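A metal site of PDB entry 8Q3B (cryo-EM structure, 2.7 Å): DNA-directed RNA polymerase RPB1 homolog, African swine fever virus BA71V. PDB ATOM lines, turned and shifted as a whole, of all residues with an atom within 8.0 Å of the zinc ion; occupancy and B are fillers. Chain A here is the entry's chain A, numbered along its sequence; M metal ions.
N of Ala 139 sits close to SG of Cys 137.
N of Cys 99 is in hydrogen-bond range of O of Ala 104, 3.1 Å away.
N of Asn 101 lies close to SG of Cys 99, 3.3 Å away.
ND2 of Asn 101 lies close to SG of Cys 137 (2.9 Å).
N of Cys 134 sits at hydrogen-bond distance from O of Ala 139, at 3.0 Å.
The side-chain sulfur (SG) of Cys 102 sits close to the backbone NH (N) of Ala 104, at 3.4 Å.
Four residues have an atom within 4 Å of the zinc ion: Cys 99, Cys 102, Cys 134 and Cys 137.
The nearest printed residue that does not touch the zinc ion is Val 136 (4.1 Å).
The zinc ion is bound by SG of Cys 99 (2.3 Å), SG of Cys 137 (2.3 Å), SG of Cys 102 (2.3 Å) and SG of Cys 134 (2.3 Å).
The zinc ion has four donor atoms within binding distance.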
ATOM      1  N   ILE A  98      14.555  30.996  20.220  1.00  0.00           N
ATOM      2  CA  ILE A  98      13.283  31.458  20.765  1.00  0.00           C
ATOM      3  C   ILE A  98      12.305  30.294  20.876  1.00  0.00           C
ATOM      4  O   ILE A  98      12.359  29.330  20.107  1.00  0.00           O
ATOM      5  CB  ILE A  98      12.698  32.599  19.907  1.00  0.00           C
ATOM      6  CG1 ILE A  98      12.279  32.086  18.518  1.00  0.00           C
ATOM      7  CG2 ILE A  98      13.696  33.737  19.789  1.00  0.00           C
ATOM      8  CD1 ILE A  98      11.006  32.685  18.000  1.00  0.00           C
ATOM      9  N   CYS A  99      11.408  30.383  21.855  1.00  0.00           N
ATOM     10  CA  CYS A  99      10.381  29.379  22.039  1.00  0.00           C
ATOM     11  C   CYS A  99       9.407  29.391  20.862  1.00  0.00           C
ATOM     12  O   CYS A  99       9.050  30.447  20.346  1.00  0.00           O
ATOM     13  CB  CYS A  99       9.630  29.621  23.344  1.00  0.00           C
ATOM     14  SG  CYS A  99       8.201  28.548  23.591  1.00  0.00           S
ATOM     15  N   LEU A 100       8.995  28.201  20.433  1.00  0.00           N
ATOM     16  CA  LEU A 100       8.088  28.084  19.296  1.00  0.00           C
ATOM     17  C   LEU A 100       6.624  28.278  19.686  1.00  0.00           C
ATOM     18  O   LEU A 100       5.793  28.508  18.789  1.00  0.00           O
ATOM     19  CB  LEU A 100       8.258  26.720  18.620  1.00  0.00           C
ATOM     20  CG  LEU A 100       9.335  26.642  17.545  1.00  0.00           C
ATOM     21  CD1 LEU A 100      10.642  27.245  18.026  1.00  0.00           C
ATOM     22  CD2 LEU A 100       9.544  25.201  17.105  1.00  0.00           C
ATOM     23  N   ASN A 101       6.291  28.196  20.965  1.00  0.00           N
ATOM     24  CA  ASN A 101       4.907  28.376  21.410  1.00  0.00           C
ATOM     25  C   ASN A 101       4.630  29.810  21.852  1.00  0.00           C
ATOM     26  O   ASN A 101       3.502  30.290  21.698  1.00  0.00           O
ATOM     27  CB  ASN A 101       4.585  27.416  22.549  1.00  0.00           C
ATOM     28  CG  ASN A 101       3.440  27.892  23.409  1.00  0.00           C
ATOM     29  OD1 ASN A 101       2.285  27.906  22.973  1.00  0.00           O
ATOM     30  ND2 ASN A 101       3.737  28.279  24.642  1.00  0.00           N
ATOM     31  N   CYS A 102       5.631  30.494  22.410  1.00  0.00           N
ATOM     32  CA  CYS A 102       5.501  31.898  22.778  1.00  0.00           C
ATOM     33  C   CYS A 102       6.687  32.676  22.237  1.00  0.00           C
ATOM     34  O   CYS A 102       7.498  32.138  21.461  1.00  0.00           O
ATOM     35  CB  CYS A 102       5.389  32.046  24.286  1.00  0.00           C
ATOM     36  SG  CYS A 102       6.938  31.777  25.175  1.00  0.00           S
ATOM     37  N   GLY A 103       6.816  33.939  22.629  1.00  0.00           N
ATOM     38  CA  GLY A 103       7.892  34.769  22.126  1.00  0.00           C
ATOM     39  C   GLY A 103       9.119  34.809  23.015  1.00  0.00           C
ATOM     40  O   GLY A 103      10.179  35.287  22.597  1.00  0.00           O
ATOM     41  N   ALA A 104       8.992  34.308  24.235  1.00  0.00           N
ATOM     42  CA  ALA A 104      10.093  34.395  25.175  1.00  0.00           C
ATOM     43  C   ALA A 104      11.265  33.529  24.702  1.00  0.00           C
ATOM     44  O   ALA A 104      11.048  32.449  24.147  1.00  0.00           O
ATOM     45  CB  ALA A 104       9.642  33.944  26.569  1.00  0.00           C
ATOM     46  N   PRO A 105      12.506  33.977  24.904  1.00  0.00           N
ATOM     47  CA  PRO A 105      13.640  33.136  24.541  1.00  0.00           C
ATOM     48  C   PRO A 105      13.843  32.000  25.528  1.00  0.00           C
ATOM     49  O   PRO A 105      13.569  32.126  26.727  1.00  0.00           O
ATOM     50  CB  PRO A 105      14.817  34.115  24.575  1.00  0.00           C
ATOM     51  CG  PRO A 105      14.425  35.133  25.568  1.00  0.00           C
ATOM     52  CD  PRO A 105      12.924  35.275  25.455  1.00  0.00           C
ATOM     53  N   ILE A 106      14.327  30.875  25.002  1.00  0.00           N
ATOM     54  CA  ILE A 106      14.615  29.719  25.846  1.00  0.00           C
ATOM     55  C   ILE A 106      16.026  29.763  26.429  1.00  0.00           C
ATOM     56  O   ILE A 106      16.286  29.077  27.434  1.00  0.00           O
ATOM     57  CB  ILE A 106      14.421  28.412  25.050  1.00  0.00           C
ATOM     58  CG1 ILE A 106      15.613  28.158  24.129  1.00  0.00           C
ATOM     59  CG2 ILE A 106      13.106  28.466  24.272  1.00  0.00           C
ATOM     60  CD1 ILE A 106      15.431  26.986  23.196  1.00  0.00           C
ATOM     61  N   GLN A 133      13.072  23.556  28.446  1.00  0.00           N
ATOM     62  CA  GLN A 133      11.709  23.978  28.754  1.00  0.00           C
ATOM     63  C   GLN A 133      11.653  25.486  28.919  1.00  0.00           C
ATOM     64  O   GLN A 133      12.493  26.090  29.591  1.00  0.00           O
ATOM     65  CB  GLN A 133      11.211  23.294  30.030  1.00  0.00           C
ATOM     66  CG  GLN A 133       9.727  23.521  30.306  1.00  0.00           C
ATOM     67  CD  GLN A 133       9.434  23.916  31.743  1.00  0.00           C
ATOM     68  OE1 GLN A 133      10.352  24.192  32.525  1.00  0.00           O
ATOM     69  NE2 GLN A 133       8.159  23.954  32.101  1.00  0.00           N
ATOM     70  N   CYS A 134      10.647  26.099  28.290  1.00  0.00           N
ATOM     71  CA  CYS A 134      10.466  27.536  28.397  1.00  0.00           C
ATOM     72  C   CYS A 134      10.028  27.916  29.811  1.00  0.00           C
ATOM     73  O   CYS A 134       9.237  27.205  30.441  1.00  0.00           O
ATOM     74  CB  CYS A 134       9.429  28.009  27.385  1.00  0.00           C
ATOM     75  SG  CYS A 134       9.513  29.773  27.003  1.00  0.00           S
ATOM     76  N   TYR A 135      10.559  29.029  30.313  1.00  0.00           N
ATOM     77  CA  TYR A 135      10.242  29.455  31.667  1.00  0.00           C
ATOM     78  C   TYR A 135       8.822  30.021  31.743  1.00  0.00           C
ATOM     79  O   TYR A 135       8.061  29.693  32.665  1.00  0.00           O
ATOM     80  CB  TYR A 135      11.256  30.489  32.148  1.00  0.00           C
ATOM     81  CG  TYR A 135      11.031  30.987  33.557  1.00  0.00           C
ATOM     82  CD1 TYR A 135      10.378  30.200  34.501  1.00  0.00           C
ATOM     83  CD2 TYR A 135      11.493  32.233  33.951  1.00  0.00           C
ATOM     84  CE1 TYR A 135      10.178  30.649  35.790  1.00  0.00           C
ATOM     85  CE2 TYR A 135      11.299  32.695  35.245  1.00  0.00           C
ATOM     86  CZ  TYR A 135      10.639  31.897  36.162  1.00  0.00           C
ATOM     87  OH  TYR A 135      10.443  32.348  37.442  1.00  0.00           O
ATOM     88  N   VAL A 136       8.449  30.861  30.782  1.00  0.00           N
ATOM     89  CA  VAL A 136       7.152  31.542  30.855  1.00  0.00           C
ATOM     90  C   VAL A 136       6.016  30.592  30.512  1.00  0.00           C
ATOM     91  O   VAL A 136       4.889  30.765  30.992  1.00  0.00           O
ATOM     92  CB  VAL A 136       7.145  32.786  29.952  1.00  0.00           C
ATOM     93  CG1 VAL A 136       8.407  33.611  30.164  1.00  0.00           C
ATOM     94  CG2 VAL A 136       7.018  32.385  28.493  1.00  0.00           C
ATOM     95  N   CYS A 137       6.260  29.588  29.677  1.00  0.00           N
ATOM     96  CA  CYS A 137       5.246  28.632  29.275  1.00  0.00           C
ATOM     97  C   CYS A 137       5.792  27.214  29.412  1.00  0.00           C
ATOM     98  O   CYS A 137       7.005  26.990  29.294  1.00  0.00           O
ATOM     99  CB  CYS A 137       4.779  28.877  27.834  1.00  0.00           C
ATOM    100  SG  CYS A 137       5.961  28.351  26.571  1.00  0.00           S
ATOM    101  N   LYS A 138       4.890  26.269  29.662  1.00  0.00           N
ATOM    102  CA  LYS A 138       5.296  24.900  29.923  1.00  0.00           C
ATOM    103  C   LYS A 138       5.818  24.179  28.686  1.00  0.00           C
ATOM    104  O   LYS A 138       6.360  23.080  28.821  1.00  0.00           O
ATOM    105  CB  LYS A 138       4.132  24.114  30.516  1.00  0.00           C
ATOM    106  CG  LYS A 138       3.606  24.662  31.844  1.00  0.00           C
ATOM    107  CD  LYS A 138       4.640  24.576  32.957  1.00  0.00           C
ATOM    108  CE  LYS A 138       4.949  23.132  33.338  1.00  0.00           C
ATOM    109  NZ  LYS A 138       5.858  23.050  34.518  1.00  0.00           N
ATOM    110  N   ALA A 139       5.668  24.770  27.502  1.00  0.00           N
ATOM    111  CA  ALA A 139       6.120  24.103  26.288  1.00  0.00           C
ATOM    112  C   ALA A 139       7.623  23.862  26.329  1.00  0.00           C
ATOM    113  O   ALA A 139       8.381  24.693  26.827  1.00  0.00           O
ATOM    114  CB  ALA A 139       5.752  24.939  25.062  1.00  0.00           C
ATOM    115  N   VAL A 140       8.043  22.720  25.804  1.00  0.00           N
ATOM    116  CA  VAL A 140       9.448  22.346  25.734  1.00  0.00           C
ATOM    117  C   VAL A 140       9.936  22.550  24.312  1.00  0.00           C
ATOM    118  O   VAL A 140       9.257  22.160  23.351  1.00  0.00           O
ATOM    119  CB  VAL A 140       9.666  20.885  26.193  1.00  0.00           C
ATOM    120  CG1 VAL A 140       9.323  19.909  25.079  1.00  0.00           C
ATOM    121  CG2 VAL A 140      11.099  20.693  26.656  1.00  0.00           C
ATOM    122  N   HIS A 141      11.104  23.164  24.167  1.00  0.00           N
ATOM    123  CA  HIS A 141      11.614  23.502  22.846  1.00  0.00           C
ATOM    124  C   HIS A 141      11.957  22.230  22.074  1.00  0.00           C
ATOM    125  O   HIS A 141      12.762  21.418  22.557  1.00  0.00           O
ATOM    126  CB  HIS A 141      12.849  24.388  22.967  1.00  0.00           C
ATOM    127  CG  HIS A 141      13.235  25.043  21.680  1.00  0.00           C
ATOM    128  ND1 HIS A 141      14.437  24.785  21.040  1.00  0.00           N
ATOM    129  CD2 HIS A 141      12.591  25.956  20.911  1.00  0.00           C
ATOM    130  CE1 HIS A 141      14.505  25.501  19.933  1.00  0.00           C
ATOM    131  NE2 HIS A 141      13.398  26.222  19.831  1.00  0.00           N
HETATM  132 ZN    ZN M   1       7.662  29.602  25.590  1.00  0.00          ZN
